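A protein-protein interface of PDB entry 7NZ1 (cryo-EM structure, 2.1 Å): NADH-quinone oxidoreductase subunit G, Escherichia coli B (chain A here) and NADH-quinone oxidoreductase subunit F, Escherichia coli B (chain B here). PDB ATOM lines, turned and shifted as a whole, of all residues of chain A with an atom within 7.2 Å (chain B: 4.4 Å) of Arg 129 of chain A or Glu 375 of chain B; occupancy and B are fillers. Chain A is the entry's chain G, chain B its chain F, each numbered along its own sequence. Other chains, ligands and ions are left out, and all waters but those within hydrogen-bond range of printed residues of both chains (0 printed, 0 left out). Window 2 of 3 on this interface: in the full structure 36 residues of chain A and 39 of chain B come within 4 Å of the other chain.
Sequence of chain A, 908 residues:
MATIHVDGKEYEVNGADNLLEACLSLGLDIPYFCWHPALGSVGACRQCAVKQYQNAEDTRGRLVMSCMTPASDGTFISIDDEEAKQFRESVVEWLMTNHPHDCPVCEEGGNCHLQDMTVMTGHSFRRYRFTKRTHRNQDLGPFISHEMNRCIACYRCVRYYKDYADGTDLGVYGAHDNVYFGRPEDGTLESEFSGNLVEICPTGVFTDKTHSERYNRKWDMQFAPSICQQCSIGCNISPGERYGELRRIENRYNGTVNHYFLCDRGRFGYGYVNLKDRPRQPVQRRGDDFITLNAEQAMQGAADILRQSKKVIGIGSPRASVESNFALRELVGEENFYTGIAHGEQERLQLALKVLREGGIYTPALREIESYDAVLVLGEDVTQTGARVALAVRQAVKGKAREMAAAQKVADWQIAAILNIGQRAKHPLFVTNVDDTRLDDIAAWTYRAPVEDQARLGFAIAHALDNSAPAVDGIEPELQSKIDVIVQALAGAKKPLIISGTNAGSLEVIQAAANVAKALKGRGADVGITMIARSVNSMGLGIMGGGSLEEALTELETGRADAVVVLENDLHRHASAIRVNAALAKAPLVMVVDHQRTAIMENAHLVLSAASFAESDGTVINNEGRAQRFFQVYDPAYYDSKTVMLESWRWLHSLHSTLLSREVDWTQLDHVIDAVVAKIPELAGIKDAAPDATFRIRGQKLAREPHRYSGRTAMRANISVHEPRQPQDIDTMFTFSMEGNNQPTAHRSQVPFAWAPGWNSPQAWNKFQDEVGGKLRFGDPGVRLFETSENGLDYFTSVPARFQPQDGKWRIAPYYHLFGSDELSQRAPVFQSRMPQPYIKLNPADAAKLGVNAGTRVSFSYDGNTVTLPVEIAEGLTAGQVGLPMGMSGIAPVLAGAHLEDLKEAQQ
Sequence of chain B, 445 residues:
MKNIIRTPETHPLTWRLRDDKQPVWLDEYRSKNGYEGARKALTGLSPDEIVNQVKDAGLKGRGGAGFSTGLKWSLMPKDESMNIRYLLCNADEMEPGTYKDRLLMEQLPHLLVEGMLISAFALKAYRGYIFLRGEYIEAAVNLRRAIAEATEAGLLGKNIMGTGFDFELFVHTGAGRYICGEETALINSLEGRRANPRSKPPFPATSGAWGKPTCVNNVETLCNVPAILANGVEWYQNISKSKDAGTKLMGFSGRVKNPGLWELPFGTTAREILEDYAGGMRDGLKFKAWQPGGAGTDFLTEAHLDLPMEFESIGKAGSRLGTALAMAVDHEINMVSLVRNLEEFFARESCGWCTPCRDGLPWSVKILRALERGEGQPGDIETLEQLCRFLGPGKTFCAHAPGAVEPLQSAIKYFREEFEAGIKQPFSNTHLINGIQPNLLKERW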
ATOM      1  N   ARG A 126      -4.462  18.788  20.576  1.00  0.00           N
ATOM      2  CA  ARG A 126      -5.576  19.004  19.661  1.00  0.00           C
ATOM      3  C   ARG A 126      -5.147  18.753  18.220  1.00  0.00           C
ATOM      4  O   ARG A 126      -4.108  19.251  17.778  1.00  0.00           O
ATOM      5  CB  ARG A 126      -6.131  20.421  19.805  1.00  0.00           C
ATOM      6  CG  ARG A 126      -7.544  20.600  19.267  1.00  0.00           C
ATOM      7  CD  ARG A 126      -8.061  22.003  19.568  1.00  0.00           C
ATOM      8  NE  ARG A 126      -9.328  22.306  18.911  1.00  0.00           N
ATOM      9  CZ  ARG A 126     -10.521  21.945  19.366  1.00  0.00           C
ATOM     10  NH1 ARG A 126     -10.656  21.243  20.479  1.00  0.00           N
ATOM     11  NH2 ARG A 126     -11.608  22.312  18.695  1.00  0.00           N
ATOM     12  N   ARG A 127      -5.959  17.980  17.493  1.00  0.00           N
ATOM     13  CA  ARG A 127      -5.794  17.741  16.064  1.00  0.00           C
ATOM     14  C   ARG A 127      -6.875  18.397  15.222  1.00  0.00           C
ATOM     15  O   ARG A 127      -6.656  18.625  14.031  1.00  0.00           O
ATOM     16  CB  ARG A 127      -5.809  16.235  15.756  1.00  0.00           C
ATOM     17  CG  ARG A 127      -4.786  15.399  16.486  1.00  0.00           C
ATOM     18  CD  ARG A 127      -4.781  13.983  15.941  1.00  0.00           C
ATOM     19  NE  ARG A 127      -5.877  13.189  16.481  1.00  0.00           N
ATOM     20  CZ  ARG A 127      -6.504  12.224  15.824  1.00  0.00           C
ATOM     21  NH1 ARG A 127      -6.165  11.895  14.589  1.00  0.00           N
ATOM     22  NH2 ARG A 127      -7.495  11.571  16.421  1.00  0.00           N
ATOM     23  N   TYR A 128      -8.029  18.674  15.811  1.00  0.00           N
ATOM     24  CA  TYR A 128      -9.165  19.236  15.099  1.00  0.00           C
ATOM     25  C   TYR A 128      -8.923  20.713  14.804  1.00  0.00           C
ATOM     26  O   TYR A 128      -8.609  21.494  15.707  1.00  0.00           O
ATOM     27  CB  TYR A 128     -10.411  19.033  15.960  1.00  0.00           C
ATOM     28  CG  TYR A 128     -11.731  19.490  15.400  1.00  0.00           C
ATOM     29  CD1 TYR A 128     -12.508  18.626  14.637  1.00  0.00           C
ATOM     30  CD2 TYR A 128     -12.232  20.758  15.678  1.00  0.00           C
ATOM     31  CE1 TYR A 128     -13.729  19.017  14.145  1.00  0.00           C
ATOM     32  CE2 TYR A 128     -13.455  21.158  15.185  1.00  0.00           C
ATOM     33  CZ  TYR A 128     -14.196  20.281  14.417  1.00  0.00           C
ATOM     34  OH  TYR A 128     -15.410  20.670  13.924  1.00  0.00           O
ATOM     35  N   ARG A 129      -9.064  21.101  13.539  1.00  0.00           N
ATOM     36  CA  ARG A 129      -8.774  22.462  13.110  1.00  0.00           C
ATOM     37  C   ARG A 129      -9.997  23.217  12.615  1.00  0.00           C
ATOM     38  O   ARG A 129      -9.870  24.379  12.215  1.00  0.00           O
ATOM     39  CB  ARG A 129      -7.700  22.458  12.014  1.00  0.00           C
ATOM     40  CG  ARG A 129      -8.159  21.962  10.650  1.00  0.00           C
ATOM     41  CD  ARG A 129      -6.993  21.887   9.681  1.00  0.00           C
ATOM     42  NE  ARG A 129      -7.375  21.377   8.371  1.00  0.00           N
ATOM     43  CZ  ARG A 129      -7.452  20.088   8.072  1.00  0.00           C
ATOM     44  NH1 ARG A 129      -7.139  19.154   8.953  1.00  0.00           N
ATOM     45  NH2 ARG A 129      -7.829  19.727   6.849  1.00  0.00           N
ATOM     46  N   PHE A 130     -11.172  22.606  12.648  1.00  0.00           N
ATOM     47  CA  PHE A 130     -12.362  23.194  12.061  1.00  0.00           C
ATOM     48  C   PHE A 130     -13.135  24.024  13.088  1.00  0.00           C
ATOM     49  O   PHE A 130     -12.711  24.205  14.229  1.00  0.00           O
ATOM     50  CB  PHE A 130     -13.213  22.092  11.443  1.00  0.00           C
ATOM     51  CG  PHE A 130     -12.447  21.205  10.504  1.00  0.00           C
ATOM     52  CD1 PHE A 130     -12.063  21.670   9.251  1.00  0.00           C
ATOM     53  CD2 PHE A 130     -12.091  19.920  10.879  1.00  0.00           C
ATOM     54  CE1 PHE A 130     -11.346  20.867   8.392  1.00  0.00           C
ATOM     55  CE2 PHE A 130     -11.374  19.104  10.020  1.00  0.00           C
ATOM     56  CZ  PHE A 130     -11.002  19.581   8.773  1.00  0.00           C
ATOM     57  N   THR A 131     -14.270  24.568  12.657  1.00  0.00           N
ATOM     58  CA  THR A 131     -15.094  25.426  13.501  1.00  0.00           C
ATOM     59  C   THR A 131     -15.836  24.632  14.574  1.00  0.00           C
ATOM     60  O   THR A 131     -16.064  23.426  14.458  1.00  0.00           O
ATOM     61  CB  THR A 131     -16.105  26.211  12.666  1.00  0.00           C
ATOM     62  OG1 THR A 131     -16.812  25.321  11.796  1.00  0.00           O
ATOM     63  CG2 THR A 131     -15.409  27.277  11.857  1.00  0.00           C
ATOM     64  N   ALA B 370     -12.742  19.345   2.990  1.00  0.00           N
ATOM     65  CA  ALA B 370     -11.382  19.823   2.748  1.00  0.00           C
ATOM     66  C   ALA B 370     -10.709  19.057   1.613  1.00  0.00           C
ATOM     67  O   ALA B 370      -9.991  19.654   0.804  1.00  0.00           O
ATOM     68  CB  ALA B 370     -10.548  19.728   4.024  1.00  0.00           C
ATOM     69  N   ARG B 373     -12.262  20.134  -1.829  1.00  0.00           N
ATOM     70  CA  ARG B 373     -11.823  21.451  -2.264  1.00  0.00           C
ATOM     71  C   ARG B 373     -10.323  21.509  -2.525  1.00  0.00           C
ATOM     72  O   ARG B 373      -9.866  22.424  -3.215  1.00  0.00           O
ATOM     73  CB  ARG B 373     -12.188  22.496  -1.214  1.00  0.00           C
ATOM     74  CG  ARG B 373     -13.658  22.831  -1.111  1.00  0.00           C
ATOM     75  CD  ARG B 373     -13.841  23.984  -0.139  1.00  0.00           C
ATOM     76  NE  ARG B 373     -13.481  23.591   1.219  1.00  0.00           N
ATOM     77  CZ  ARG B 373     -14.346  23.164   2.129  1.00  0.00           C
ATOM     78  NH1 ARG B 373     -15.642  23.089   1.870  1.00  0.00           N
ATOM     79  NH2 ARG B 373     -13.900  22.805   3.329  1.00  0.00           N
ATOM     80  N   GLY B 374      -9.558  20.542  -2.023  1.00  0.00           N
ATOM     81  CA  GLY B 374      -8.117  20.560  -2.149  1.00  0.00           C
ATOM     82  C   GLY B 374      -7.371  21.188  -0.994  1.00  0.00           C
ATOM     83  O   GLY B 374      -6.172  21.449  -1.126  1.00  0.00           O
ATOM     84  N   GLU B 375      -8.035  21.429   0.135  1.00  0.00           N
ATOM     85  CA  GLU B 375      -7.418  22.002   1.324  1.00  0.00           C
ATOM     86  C   GLU B 375      -6.989  20.957   2.349  1.00  0.00           C
ATOM     87  O   GLU B 375      -6.713  21.319   3.497  1.00  0.00           O
ATOM     88  CB  GLU B 375      -8.360  23.016   1.980  1.00  0.00           C
ATOM     89  CG  GLU B 375      -8.424  24.366   1.287  1.00  0.00           C
ATOM     90  CD  GLU B 375      -9.384  24.414   0.123  1.00  0.00           C
ATOM     91  OE1 GLU B 375      -8.978  24.043  -0.995  1.00  0.00           O
ATOM     92  OE2 GLU B 375     -10.527  24.878   0.319  1.00  0.00           O
ATOM     93  N   GLY B 376      -6.986  19.677   1.979  1.00  0.00           N
ATOM     94  CA  GLY B 376      -6.606  18.623   2.911  1.00  0.00           C
ATOM     95  C   GLY B 376      -5.144  18.690   3.334  1.00  0.00           C
ATOM     96  O   GLY B 376      -4.260  19.039   2.552  1.00  0.00           O
ATOM     97  N   GLN B 377      -4.904  18.364   4.598  1.00  0.00           N
ATOM     98  CA  GLN B 377      -3.645  18.336   5.331  1.00  0.00           C
ATOM     99  C   GLN B 377      -3.145  16.898   5.469  1.00  0.00           C
ATOM    100  O   GLN B 377      -3.941  15.964   5.366  1.00  0.00           O
ATOM    101  CB  GLN B 377      -3.868  19.001   6.693  1.00  0.00           C
ATOM    102  CG  GLN B 377      -4.285  20.450   6.526  1.00  0.00           C
ATOM    103  CD  GLN B 377      -4.042  21.278   7.754  1.00  0.00           C
ATOM    104  OE1 GLN B 377      -3.693  20.752   8.809  1.00  0.00           O
ATOM    105  NE2 GLN B 377      -4.209  22.590   7.626  1.00  0.00           N
ATOM    106  N   ASP B 380      -4.922  13.953   7.504  1.00  0.00           N
ATOM    107  CA  ASP B 380      -6.372  13.836   7.353  1.00  0.00           C
ATOM    108  C   ASP B 380      -6.828  12.423   7.004  1.00  0.00           C
ATOM    109  O   ASP B 380      -7.858  11.966   7.512  1.00  0.00           O
ATOM    110  CB  ASP B 380      -6.864  14.810   6.283  1.00  0.00           C
ATOM    111  CG  ASP B 380      -7.081  16.209   6.824  1.00  0.00           C
ATOM    112  OD1 ASP B 380      -6.620  16.485   7.949  1.00  0.00           O
ATOM    113  OD2 ASP B 380      -7.702  17.030   6.123  1.00  0.00           O
ATOM    114  N   GLY B 422      -6.403  15.131  -2.788  1.00  0.00           N
ATOM    115  CA  GLY B 422      -6.856  16.241  -1.967  1.00  0.00           C
ATOM    116  C   GLY B 422      -5.791  16.873  -1.088  1.00  0.00           C
ATOM    117  O   GLY B 422      -5.941  18.034  -0.697  1.00  0.00           O
ATOM    118  N   GLN B 425      -2.006  20.899   1.072  1.00  0.00           N
ATOM    119  CA  GLN B 425      -1.607  21.910   2.037  1.00  0.00           C
ATOM    120  C   GLN B 425      -0.982  21.218   3.239  1.00  0.00           C
ATOM    121  O   GLN B 425      -1.371  20.096   3.573  1.00  0.00           O
ATOM    122  CB  GLN B 425      -2.816  22.757   2.485  1.00  0.00           C
ATOM    123  CG  GLN B 425      -3.579  23.425   1.344  1.00  0.00           C
ATOM    124  CD  GLN B 425      -4.477  24.555   1.796  1.00  0.00           C
ATOM    125  OE1 GLN B 425      -4.570  24.858   2.984  1.00  0.00           O
ATOM    126  NE2 GLN B 425      -5.159  25.177   0.844  1.00  0.00           N
ATOM    127  N   ASN B 429      -2.678  23.883  12.664  1.00  0.00           N
ATOM    128  CA  ASN B 429      -3.930  24.168  13.357  1.00  0.00           C
ATOM    129  C   ASN B 429      -3.745  25.213  14.450  1.00  0.00           C
ATOM    130  O   ASN B 429      -4.610  25.362  15.315  1.00  0.00           O
ATOM    131  CB  ASN B 429      -4.551  22.894  13.943  1.00  0.00           C
ATOM    132  CG  ASN B 429      -3.624  22.156  14.906  1.00  0.00           C
ATOM    133  OD1 ASN B 429      -2.448  22.485  15.051  1.00  0.00           O
ATOM    134  ND2 ASN B 429      -4.173  21.163  15.589  1.00  0.00           N
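The side-chain amide nitrogen (NE2) of Gln 377 of chain B sits close to the guanidinium group (NE) of Arg 129 of chain A. The guanidinium group (NH2) of Arg 129 of chain A is in salt-bridge range of the side-chain carboxylate (OD2) of Asp 380 of chain B (2.8 Å). The side-chain amide nitrogen (ND2) of Asn 429 of chain B is in hydrogen-bond range of the backbone carbonyl oxygen (O) of Arg 126 of chain A (2.9 Å).
O of Ala 370 of chain B is in hydrogen-bond range of N of Glu 375 of chain B. N of Gly 376 of chain B is in hydrogen-bond range of O of Ala 370 of chain B. OE2 of Glu 375 of chain B is in salt-bridge range of NE of Arg 373 of chain B, at 3.3 Å. The backbone NH (N) of Gln 377 of chain B is in hydrogen-bond range of the side-chain carboxylate (OD2) of Asp 380 of chain B (3.5 Å). O of Tyr 128 of chain A is in hydrogen-bond range of NE of Arg 126 of chain A.
CA of Arg 127 of chain A touches ND2 of Asn 429 of chain B (3.8 Å). NH2 of Arg 129 of chain A touches CB of Ala 370 of chain B, 3.9 Å away. Glu 375 of chain B touches Arg 129 of chain A (O to NH2, 3.9 Å). Asn 429 of chain B touches Arg 129 of chain A.
Of the printed residues of chain B, Arg 126 of chain A touches Asn 429 (2.9 Å). Of the printed residues of chain B, Arg 129 of chain A touches Ala 370 (3.9 Å), Glu 375 (3.9 Å), Gln 377 (3.4 Å), Asp 380 (2.8 Å) and Asn 429 (3.7 Å). Of the printed residues of chain A, Ala 370 of chain B touches Arg 129 (3.9 Å). Glu 375 of chain B touches just one residue of chain A: Arg 129. Of the printed residues of chain A, Gln 377 of chain B touches Arg 129 (3.4 Å). Printed residues of chain A within 4 Å of Asp 380 of chain B: Arg 129. The nearest residue of chain B that does not touch Arg 129 of chain A is Gly 376 of chain B (4.3 Å). The nearest residue of chain A that does not touch Glu 375 of chain B is Phe 130 of chain A (6.8 Å). The nearest printed residue of chain B that does not touch Arg 126 of chain A is Gln 377 of chain B (9.1 Å).
Printed residues of chain B that touch a printed residue of chain A: Ala 370, Glu 375, Gln 377, Asp 380 and Asn 429. Along chain B the printed residues that touch a printed residue of chain A span positions 370 to 429. Among the printed residues, Asp or Glu carboxylates within 4 Å of a Lys or Arg side-chain nitrogen of the other chain: Arg 129 of chain A with Asp 380 of chain B.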
